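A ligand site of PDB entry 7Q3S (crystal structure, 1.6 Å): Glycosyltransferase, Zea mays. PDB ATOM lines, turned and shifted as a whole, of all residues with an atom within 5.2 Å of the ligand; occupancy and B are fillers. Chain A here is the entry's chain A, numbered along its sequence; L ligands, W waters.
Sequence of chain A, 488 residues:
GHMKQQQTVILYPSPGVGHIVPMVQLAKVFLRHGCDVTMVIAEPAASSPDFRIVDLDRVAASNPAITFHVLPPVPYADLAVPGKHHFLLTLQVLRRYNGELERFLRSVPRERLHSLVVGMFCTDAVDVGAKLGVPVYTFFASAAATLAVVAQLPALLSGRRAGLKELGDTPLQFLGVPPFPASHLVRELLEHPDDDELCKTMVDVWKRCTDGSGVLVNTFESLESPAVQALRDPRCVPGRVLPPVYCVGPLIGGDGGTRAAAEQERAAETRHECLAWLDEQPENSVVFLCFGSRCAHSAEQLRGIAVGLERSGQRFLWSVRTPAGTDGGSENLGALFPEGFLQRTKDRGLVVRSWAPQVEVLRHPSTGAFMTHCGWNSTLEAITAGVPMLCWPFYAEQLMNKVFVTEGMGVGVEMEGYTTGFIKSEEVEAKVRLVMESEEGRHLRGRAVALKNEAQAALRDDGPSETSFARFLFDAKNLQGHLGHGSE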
ATOM      1  N   VAL A  17     -33.149  -1.560   2.296  1.00  0.00           N
ATOM      2  CA  VAL A  17     -32.708  -2.848   1.760  1.00  0.00           C
ATOM      3  C   VAL A  17     -31.483  -3.326   2.508  1.00  0.00           C
ATOM      4  O   VAL A  17     -31.344  -4.507   2.785  1.00  0.00           O
ATOM      5  CB  VAL A  17     -32.424  -2.721   0.242  1.00  0.00           C
ATOM      6  CG1 VAL A  17     -31.910  -4.056  -0.377  1.00  0.00           C
ATOM      7  CG2 VAL A  17     -33.596  -2.244  -0.529  1.00  0.00           C
ATOM      8  N   GLY A  18     -30.561  -2.434   2.835  1.00  0.00           N
ATOM      9  CA  GLY A  18     -29.264  -2.772   3.413  1.00  0.00           C
ATOM     10  C   GLY A  18     -29.329  -3.200   4.851  1.00  0.00           C
ATOM     11  O   GLY A  18     -28.375  -3.750   5.398  1.00  0.00           O
ATOM     12  N   VAL A  21     -32.335  -6.888   4.221  1.00  0.00           N
ATOM     13  CA  VAL A  21     -31.826  -8.051   3.488  1.00  0.00           C
ATOM     14  C   VAL A  21     -30.832  -8.855   4.330  1.00  0.00           C
ATOM     15  O   VAL A  21     -31.000 -10.085   4.459  1.00  0.00           O
ATOM     16  CB  VAL A  21     -31.226  -7.631   2.155  1.00  0.00           C
ATOM     17  CG1 VAL A  21     -30.289  -8.735   1.616  1.00  0.00           C
ATOM     18  CG2 VAL A  21     -32.348  -7.334   1.167  1.00  0.00           C
ATOM     19  N   CYS A 290     -23.408  -1.054 -10.816  1.00  0.00           N
ATOM     20  CA  CYS A 290     -24.664  -1.058 -10.085  1.00  0.00           C
ATOM     21  C   CYS A 290     -24.482  -0.282  -8.777  1.00  0.00           C
ATOM     22  O   CYS A 290     -23.540  -0.524  -8.023  1.00  0.00           O
ATOM     23  CB  CYS A 290     -25.064  -2.524  -9.839  1.00  0.00           C
ATOM     24  SG  CYS A 290     -26.759  -2.737  -9.330  1.00  0.00           S
ATOM     25  N   GLY A 292     -26.298   0.655  -5.649  1.00  0.00           N
ATOM     26  CA  GLY A 292     -27.121   0.707  -4.456  1.00  0.00           C
ATOM     27  C   GLY A 292     -28.610   0.622  -4.696  1.00  0.00           C
ATOM     28  O   GLY A 292     -29.148   0.524  -5.783  1.00  0.00           O
ATOM     29  N   SER A 293     -29.288   0.598  -3.559  1.00  0.00           N
ATOM     30  CA  SER A 293     -30.719   0.473  -3.634  1.00  0.00           C
ATOM     31  C   SER A 293     -31.361   1.759  -4.081  1.00  0.00           C
ATOM     32  O   SER A 293     -32.534   1.751  -4.492  1.00  0.00           O
ATOM     33  CB  SER A 293     -31.268  -0.007  -2.277  1.00  0.00           C
ATOM     34  OG  SER A 293     -31.123   0.980  -1.294  1.00  0.00           O
ATOM     35  N   ARG A 294     -30.656   2.903  -3.981  1.00  0.00           N
ATOM     36  CA  ARG A 294     -31.345   4.092  -4.438  1.00  0.00           C
ATOM     37  C   ARG A 294     -30.470   5.202  -5.029  1.00  0.00           C
ATOM     38  O   ARG A 294     -31.020   6.224  -5.363  1.00  0.00           O
ATOM     39  CB  ARG A 294     -32.211   4.705  -3.347  1.00  0.00           C
ATOM     40  CG  ARG A 294     -31.907   4.407  -1.974  1.00  0.00           C
ATOM     41  CD  ARG A 294     -32.854   5.190  -1.080  1.00  0.00           C
ATOM     42  NE  ARG A 294     -32.567   5.049   0.332  1.00  0.00           N
ATOM     43  CZ  ARG A 294     -31.865   5.906   1.073  1.00  0.00           C
ATOM     44  NH1 ARG A 294     -31.317   6.997   0.553  1.00  0.00           N
ATOM     45  NH2 ARG A 294     -31.705   5.645   2.379  1.00  0.00           N
ATOM     46  N   SER A 319     -26.557  -1.682 -14.801  1.00  0.00           N
ATOM     47  CA  SER A 319     -27.892  -1.468 -14.228  1.00  0.00           C
ATOM     48  C   SER A 319     -28.088   0.045 -14.066  1.00  0.00           C
ATOM     49  O   SER A 319     -27.358   0.696 -13.288  1.00  0.00           O
ATOM     50  CB  SER A 319     -28.081  -2.160 -12.862  1.00  0.00           C
ATOM     51  OG  SER A 319     -29.439  -2.003 -12.523  1.00  0.00           O
ATOM     52  N   ARG A 321     -30.585   3.412 -13.381  1.00  0.00           N
ATOM     53  CA  ARG A 321     -31.829   4.042 -12.924  1.00  0.00           C
ATOM     54  C   ARG A 321     -32.131   5.319 -13.704  1.00  0.00           C
ATOM     55  O   ARG A 321     -31.208   6.100 -13.973  1.00  0.00           O
ATOM     56  CB  ARG A 321     -31.772   4.475 -11.468  1.00  0.00           C
ATOM     57  CG  ARG A 321     -31.587   3.477 -10.505  1.00  0.00           C
ATOM     58  CD  ARG A 321     -32.065   3.896  -9.088  1.00  0.00           C
ATOM     59  NE  ARG A 321     -32.213   2.585  -8.457  1.00  0.00           N
ATOM     60  CZ  ARG A 321     -31.242   1.937  -7.831  1.00  0.00           C
ATOM     61  NH1 ARG A 321     -30.057   2.484  -7.643  1.00  0.00           N
ATOM     62  NH2 ARG A 321     -31.482   0.694  -7.385  1.00  0.00           N
ATOM     63  N   SER A 354     -32.838  -0.398 -13.782  1.00  0.00           N
ATOM     64  CA  SER A 354     -33.315  -0.133 -12.431  1.00  0.00           C
ATOM     65  C   SER A 354     -32.913  -1.137 -11.374  1.00  0.00           C
ATOM     66  O   SER A 354     -32.396  -0.674 -10.345  1.00  0.00           O
ATOM     67  CB  SER A 354     -34.849   0.001 -12.367  1.00  0.00           C
ATOM     68  OG  SER A 354     -35.413  -1.296 -12.257  1.00  0.00           O
ATOM     69  N   TRP A 355     -33.236  -2.458 -11.513  1.00  0.00           N
ATOM     70  CA  TRP A 355     -32.882  -3.428 -10.437  1.00  0.00           C
ATOM     71  C   TRP A 355     -32.326  -4.719 -11.035  1.00  0.00           C
ATOM     72  O   TRP A 355     -33.047  -5.478 -11.691  1.00  0.00           O
ATOM     73  CB  TRP A 355     -34.080  -3.817  -9.529  1.00  0.00           C
ATOM     74  CG  TRP A 355     -33.622  -4.504  -8.241  1.00  0.00           C
ATOM     75  CD1 TRP A 355     -33.447  -5.873  -7.997  1.00  0.00           C
ATOM     76  CD2 TRP A 355     -33.276  -3.859  -7.023  1.00  0.00           C
ATOM     77  NE1 TRP A 355     -32.972  -6.060  -6.744  1.00  0.00           N
ATOM     78  CE2 TRP A 355     -32.874  -4.851  -6.111  1.00  0.00           C
ATOM     79  CE3 TRP A 355     -33.240  -2.522  -6.601  1.00  0.00           C
ATOM     80  CZ2 TRP A 355     -32.444  -4.540  -4.841  1.00  0.00           C
ATOM     81  CZ3 TRP A 355     -32.793  -2.226  -5.321  1.00  0.00           C
ATOM     82  CH2 TRP A 355     -32.441  -3.248  -4.456  1.00  0.00           C
ATOM     83  N   ALA A 356     -31.071  -4.985 -10.701  1.00  0.00           N
ATOM     84  CA  ALA A 356     -30.338  -6.099 -11.226  1.00  0.00           C
ATOM     85  C   ALA A 356     -30.109  -7.167 -10.137  1.00  0.00           C
ATOM     86  O   ALA A 356     -30.169  -6.863  -8.940  1.00  0.00           O
ATOM     87  CB  ALA A 356     -28.976  -5.644 -11.756  1.00  0.00           C
ATOM     88  N   PRO A 357     -29.930  -8.479 -10.560  1.00  0.00           N
ATOM     89  CA  PRO A 357     -29.586  -9.531  -9.586  1.00  0.00           C
ATOM     90  C   PRO A 357     -28.136  -9.452  -9.117  1.00  0.00           C
ATOM     91  O   PRO A 357     -27.277 -10.213  -9.585  1.00  0.00           O
ATOM     92  CB  PRO A 357     -29.908 -10.798 -10.400  1.00  0.00           C
ATOM     93  CG  PRO A 357     -29.468 -10.415 -11.834  1.00  0.00           C
ATOM     94  CD  PRO A 357     -29.935  -8.968 -11.945  1.00  0.00           C
ATOM     95  N   GLN A 358     -27.833  -8.422  -8.292  1.00  0.00           N
ATOM     96  CA  GLN A 358     -26.450  -8.063  -8.034  1.00  0.00           C
ATOM     97  C   GLN A 358     -25.635  -9.191  -7.425  1.00  0.00           C
ATOM     98  O   GLN A 358     -24.491  -9.446  -7.839  1.00  0.00           O
ATOM     99  CB  GLN A 358     -26.393  -6.805  -7.169  1.00  0.00           C
ATOM    100  CG  GLN A 358     -25.040  -6.563  -6.548  1.00  0.00           C
ATOM    101  CD  GLN A 358     -24.854  -5.160  -5.985  1.00  0.00           C
ATOM    102  OE1 GLN A 358     -25.300  -4.183  -6.603  1.00  0.00           O
ATOM    103  NE2 GLN A 358     -24.219  -5.058  -4.838  1.00  0.00           N
ATOM    104  N   VAL A 359     -26.164  -9.866  -6.393  1.00  0.00           N
ATOM    105  CA  VAL A 359     -25.360 -10.887  -5.740  1.00  0.00           C
ATOM    106  C   VAL A 359     -24.962 -11.982  -6.756  1.00  0.00           C
ATOM    107  O   VAL A 359     -23.803 -12.420  -6.799  1.00  0.00           O
ATOM    108  CB  VAL A 359     -26.142 -11.465  -4.555  1.00  0.00           C
ATOM    109  CG1 VAL A 359     -25.519 -12.768  -4.151  1.00  0.00           C
ATOM    110  CG2 VAL A 359     -26.105 -10.570  -3.371  1.00  0.00           C
ATOM    111  N   HIS A 373     -21.223   1.846  -5.576  1.00  0.00           N
ATOM    112  CA  HIS A 373     -21.377   2.981  -4.638  1.00  0.00           C
ATOM    113  C   HIS A 373     -20.795   2.745  -3.238  1.00  0.00           C
ATOM    114  O   HIS A 373     -20.779   3.647  -2.409  1.00  0.00           O
ATOM    115  CB  HIS A 373     -22.872   3.357  -4.561  1.00  0.00           C
ATOM    116  CG  HIS A 373     -23.647   2.553  -3.555  1.00  0.00           C
ATOM    117  ND1 HIS A 373     -23.670   1.174  -3.500  1.00  0.00           N
ATOM    118  CD2 HIS A 373     -24.448   2.981  -2.535  1.00  0.00           C
ATOM    119  CE1 HIS A 373     -24.452   0.783  -2.506  1.00  0.00           C
ATOM    120  NE2 HIS A 373     -24.927   1.867  -1.896  1.00  0.00           N
ATOM    121  N   GLY A 375     -21.661   0.900  -0.767  1.00  0.00           N
ATOM    122  CA  GLY A 375     -22.457   0.432   0.380  1.00  0.00           C
ATOM    123  C   GLY A 375     -21.839  -0.826   0.978  1.00  0.00           C
ATOM    124  O   GLY A 375     -21.194  -1.599   0.306  1.00  0.00           O
ATOM    125  N   TRP A 376     -22.126  -1.074   2.254  1.00  0.00           N
ATOM    126  CA  TRP A 376     -21.419  -2.179   2.902  1.00  0.00           C
ATOM    127  C   TRP A 376     -21.896  -3.522   2.362  1.00  0.00           C
ATOM    128  O   TRP A 376     -21.086  -4.417   2.214  1.00  0.00           O
ATOM    129  CB  TRP A 376     -21.544  -2.098   4.428  1.00  0.00           C
ATOM    130  CG  TRP A 376     -20.660  -3.160   5.073  1.00  0.00           C
ATOM    131  CD1 TRP A 376     -21.098  -4.229   5.839  1.00  0.00           C
ATOM    132  CD2 TRP A 376     -19.235  -3.306   4.969  1.00  0.00           C
ATOM    133  NE1 TRP A 376     -20.056  -4.994   6.225  1.00  0.00           N
ATOM    134  CE2 TRP A 376     -18.891  -4.464   5.729  1.00  0.00           C
ATOM    135  CE3 TRP A 376     -18.208  -2.557   4.376  1.00  0.00           C
ATOM    136  CZ2 TRP A 376     -17.571  -4.892   5.867  1.00  0.00           C
ATOM    137  CZ3 TRP A 376     -16.874  -3.024   4.523  1.00  0.00           C
ATOM    138  CH2 TRP A 376     -16.573  -4.197   5.226  1.00  0.00           C
ATOM    139  N   ASN A 377     -23.200  -3.711   2.175  1.00  0.00           N
ATOM    140  CA  ASN A 377     -23.630  -5.005   1.606  1.00  0.00           C
ATOM    141  C   ASN A 377     -22.988  -5.225   0.246  1.00  0.00           C
ATOM    142  O   ASN A 377     -22.506  -6.294  -0.024  1.00  0.00           O
ATOM    143  CB  ASN A 377     -25.125  -5.159   1.536  1.00  0.00           C
ATOM    144  CG  ASN A 377     -25.721  -5.166   2.910  1.00  0.00           C
ATOM    145  OD1 ASN A 377     -25.681  -6.198   3.602  1.00  0.00           O
ATOM    146  ND2 ASN A 377     -26.346  -4.047   3.317  1.00  0.00           N
ATOM    147  N   SER A 378     -22.960  -4.188  -0.594  1.00  0.00           N
ATOM    148  CA  SER A 378     -22.365  -4.322  -1.910  1.00  0.00           C
ATOM    149  C   SER A 378     -20.887  -4.652  -1.800  1.00  0.00           C
ATOM    150  O   SER A 378     -20.368  -5.477  -2.593  1.00  0.00           O
ATOM    151  CB  SER A 378     -22.553  -3.028  -2.701  1.00  0.00           C
ATOM    152  OG  SER A 378     -23.910  -2.769  -2.999  1.00  0.00           O
ATOM    153  N   THR A 379     -20.202  -4.023  -0.889  1.00  0.00           N
ATOM    154  CA  THR A 379     -18.780  -4.260  -0.628  1.00  0.00           C
ATOM    155  C   THR A 379     -18.555  -5.693  -0.182  1.00  0.00           C
ATOM    156  O   THR A 379     -17.726  -6.415  -0.734  1.00  0.00           O
ATOM    157  CB  THR A 379     -18.219  -3.280   0.394  1.00  0.00           C
ATOM    158  OG1 THR A 379     -18.394  -1.927  -0.041  1.00  0.00           O
ATOM    159  CG2 THR A 379     -16.784  -3.470   0.700  1.00  0.00           C
ATOM    160  N   GLU A 381     -20.564  -8.265  -0.702  1.00  0.00           N
ATOM    161  CA  GLU A 381     -20.915  -9.114  -1.824  1.00  0.00           C
ATOM    162  C   GLU A 381     -19.743  -9.251  -2.787  1.00  0.00           C
ATOM    163  O   GLU A 381     -19.417 -10.348  -3.222  1.00  0.00           O
ATOM    164  CB  GLU A 381     -22.159  -8.549  -2.506  1.00  0.00           C
ATOM    165  CG  GLU A 381     -23.421  -8.759  -1.560  1.00  0.00           C
ATOM    166  CD  GLU A 381     -24.594  -7.909  -1.968  1.00  0.00           C
ATOM    167  OE1 GLU A 381     -24.553  -7.274  -3.024  1.00  0.00           O
ATOM    168  OE2 GLU A 381     -25.601  -7.913  -1.172  1.00  0.00           O
ATOM    169  N   TYR A 395     -22.883   8.560  -0.274  1.00  0.00           N
ATOM    170  CA  TYR A 395     -23.459   9.077   0.960  1.00  0.00           C
ATOM    171  C   TYR A 395     -23.311   8.058   2.088  1.00  0.00           C
ATOM    172  O   TYR A 395     -22.636   7.034   1.937  1.00  0.00           O
ATOM    173  CB  TYR A 395     -24.953   9.493   0.753  1.00  0.00           C
ATOM    174  CG  TYR A 395     -25.927   8.352   0.537  1.00  0.00           C
ATOM    175  CD1 TYR A 395     -26.501   7.660   1.630  1.00  0.00           C
ATOM    176  CD2 TYR A 395     -26.367   8.006  -0.737  1.00  0.00           C
ATOM    177  CE1 TYR A 395     -27.415   6.615   1.432  1.00  0.00           C
ATOM    178  CE2 TYR A 395     -27.273   6.961  -0.951  1.00  0.00           C
ATOM    179  CZ  TYR A 395     -27.803   6.284   0.140  1.00  0.00           C
ATOM    180  OH  TYR A 395     -28.727   5.252  -0.025  1.00  0.00           O
ATOM    181  N   GLN A 398     -20.368   5.384   2.920  1.00  0.00           N
ATOM    182  CA  GLN A 398     -19.796   4.864   1.677  1.00  0.00           C
ATOM    183  C   GLN A 398     -18.424   5.452   1.393  1.00  0.00           C
ATOM    184  O   GLN A 398     -17.561   4.770   0.891  1.00  0.00           O
ATOM    185  CB  GLN A 398     -20.731   5.145   0.496  1.00  0.00           C
ATOM    186  CG  GLN A 398     -22.034   4.404   0.520  1.00  0.00           C
ATOM    187  CD  GLN A 398     -23.138   5.101  -0.148  1.00  0.00           C
ATOM    188  OE1 GLN A 398     -22.969   5.882  -1.052  1.00  0.00           O
ATOM    189  NE2 GLN A 398     -24.348   4.779   0.283  1.00  0.00           N
HETATM  190  N1  LIG L   1     -29.062  -4.454  -4.913  1.00  0.00           N
HETATM  191  C1  LIG L   1     -29.521  -5.373  -5.901  1.00  0.00           C
HETATM  192  N2  LIG L   1     -29.775  -4.888  -7.221  1.00  0.00           N
HETATM  193  C2  LIG L   1     -29.659  -3.511  -7.561  1.00  0.00           C
HETATM  194  C3  LIG L   1     -29.180  -2.583  -6.563  1.00  0.00           C
HETATM  195  C4  LIG L   1     -28.876  -3.095  -5.208  1.00  0.00           C
HETATM  196  O1  LIG L   1     -29.673  -6.536  -5.713  1.00  0.00           O
HETATM  197  O2  LIG L   1     -29.913  -3.203  -8.716  1.00  0.00           O
HETATM  198  C5  LIG L   1     -28.829  -4.934  -3.539  1.00  0.00           C
HETATM  199  C6  LIG L   1     -27.322  -5.224  -3.342  1.00  0.00           C
HETATM  200  O3  LIG L   1     -27.024  -6.477  -3.806  1.00  0.00           O
HETATM  201  C7  LIG L   1     -27.249  -4.954  -1.852  1.00  0.00           C
HETATM  202  C8  LIG L   1     -28.181  -4.016  -1.563  1.00  0.00           C
HETATM  203  O4  LIG L   1     -29.164  -3.897  -2.797  1.00  0.00           O
HETATM  204  O5  LIG L   1     -27.572  -6.228  -1.088  1.00  0.00           O
HETATM  205  C9  LIG L   1     -27.662  -2.640  -1.370  1.00  0.00           C
HETATM  206  O6  LIG L   1     -27.167  -2.552  -0.062  1.00  0.00           O
HETATM  207  P1  LIG L   1     -25.873  -1.655   0.286  1.00  0.00           P
HETATM  208  O7  LIG L   1     -24.770  -1.881  -0.588  1.00  0.00           O
HETATM  209  O8  LIG L   1     -25.571  -1.804   1.739  1.00  0.00           O
HETATM  210  O9  LIG L   1     -26.228  -0.135   0.049  1.00  0.00           O
HETATM  211  P2  LIG L   1     -27.594   0.824   0.229  1.00  0.00           P
HETATM  212  O10 LIG L   1     -28.572   0.544  -0.870  1.00  0.00           O
HETATM  213  O11 LIG L   1     -28.077   0.623   1.620  1.00  0.00           O
HETATM  214  O12 LIG L   1     -27.028   2.167   0.053  1.00  0.00           O
HETATM  215  O   HOH W   1     -30.373   0.386   2.602  1.00  0.00           O
HETATM  216  O   HOH W   2     -28.756  -9.016  -5.032  1.00  0.00           O
HETATM  217  O   HOH W   3     -29.710  -0.784 -10.029  1.00  0.00           O
HETATM  218  O   HOH W   4     -25.726  -1.993  -5.134  1.00  0.00           O
HETATM  219  O   HOH W   5     -28.402   3.335  -2.260  1.00  0.00           O
HETATM  220  O   HOH W   6     -25.210   2.906   2.215  1.00  0.00           O
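O5 of the ligand is in hydrogen-bond range of OE2 of Glu 381 (2.6 Å).
The backbone NH (N) of Ser 293 sits at hydrogen-bond distance from an oxygen (O10) of the ligand (2.8 Å).
The side-chain hydroxyl of Ser 293 sits at hydrogen-bond distance from an oxygen (O10) of the ligand.
The backbone NH of Ala 356 is in hydrogen-bond range of an oxygen (O2) of the ligand.
The backbone carbonyl oxygen (O) of Ala 356 is in hydrogen-bond range of a nitrogen (N2) of the ligand (2.6 Å).
N of Ser 378 lies within hydrogen-bond range of O7 of the ligand, at 2.9 Å.
OG of Ser 378 sits at hydrogen-bond distance from O7 of the ligand, at 2.7 Å.
The backbone NH (N) of Asn 377 lies within hydrogen-bond range of an oxygen (O8) of the ligand (3.1 Å).
The side-chain amide nitrogen (ND2) of Asn 377 sits at hydrogen-bond distance from an oxygen (O8) of the ligand (2.8 Å).
A ring nitrogen (NE2) of His 373 lies within hydrogen-bond range of an oxygen (O12) of the ligand (2.9 Å).
An oxygen (O1) of the ligand lies within hydrogen-bond range of the indole nitrogen (NE1) of Trp 355, at 3.5 Å.
An oxygen (O2) of the ligand lies within hydrogen-bond range of the side-chain sulfur (SG) of Cys 290 (3.2 Å).
NE2 of Gln 358 is in hydrogen-bond range of O3 of the ligand (3.3 Å).
The backbone carbonyl oxygen (O) of Ser 293 is in hydrogen-bond range of the guanidinium group (NH2) of Arg 321.
ND2 of Asn 377 sits at hydrogen-bond distance from O of Gly 18 (2.9 Å).
The backbone NH (N) of Gly 292 sits at hydrogen-bond distance from a ring nitrogen (ND1) of His 373 (3.4 Å).
OE1 of Gln 398 lies close to O of His 373.
NH2 of Arg 321 is in hydrogen-bond range of O of Gly 292 (2.8 Å).
The side-chain sulfur (SG) of Cys 290 sits at hydrogen-bond distance from the side-chain amide oxygen (OE1) of Gln 358 (3.4 Å).
O of Gly 375 sits at hydrogen-bond distance from OG1 of Thr 379 (2.8 Å).
The backbone carbonyl oxygen (O) of Ser 354 lies within hydrogen-bond range of the guanidinium group (NH2) of Arg 321, 3.4 Å away.
Val 17 touches the ligand.
Gly 292 touches the ligand.
O of Ser 354 touches O2 of the ligand (3.9 Å).
CA of Gly 375 touches O7 of the ligand, at 3.4 Å.
Trp 376 touches the ligand.
Tyr 395 touches the ligand.
Gln 398 touches the ligand (NE2 to O12, 3.7 Å).
16 residues have an atom within 4 Å of the ligand: Val 17, Cys 290, Gly 292, Ser 293, Ser 354, Trp 355, Ala 356, Gln 358, His 373, Gly 375, Trp 376, Asn 377, Ser 378, Glu 381, Tyr 395 and Gln 398.
The nearest printed residue that does not touch the ligand is Gly 18 (4.02 Å).
Water W1 lies within hydrogen-bond range of O11 of the ligand, N of Gly 18 and N of Val 17.
Water W2 lies within hydrogen-bond range of O1 of the ligand, N of Val 359 and N of Gln 358.
Water W3 lies within hydrogen-bond range of the backbone carbonyl oxygen (O) of Ser 354, an oxygen (O2) of the ligand, the side-chain hydroxyl (OG) of Ser 319 and the side-chain sulfur (SG) of Cys 290.
Water W6 bridges NE2 of Gln 398 (2.8 Å) and O12 of the ligand (2.9 Å).
Water W5 lies within hydrogen-bond range of N of Arg 294 (2.9 Å), O12 of the ligand (2.9 Å), OH of Tyr 395 (3.0 Å) and N of Ser 293 (3.2 Å).
Water W4 lies within hydrogen-bond range of OE1 of Gln 358 (2.7 Å), N of Gly 292 (2.8 Å) and OG of Ser 378 (2.9 Å).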
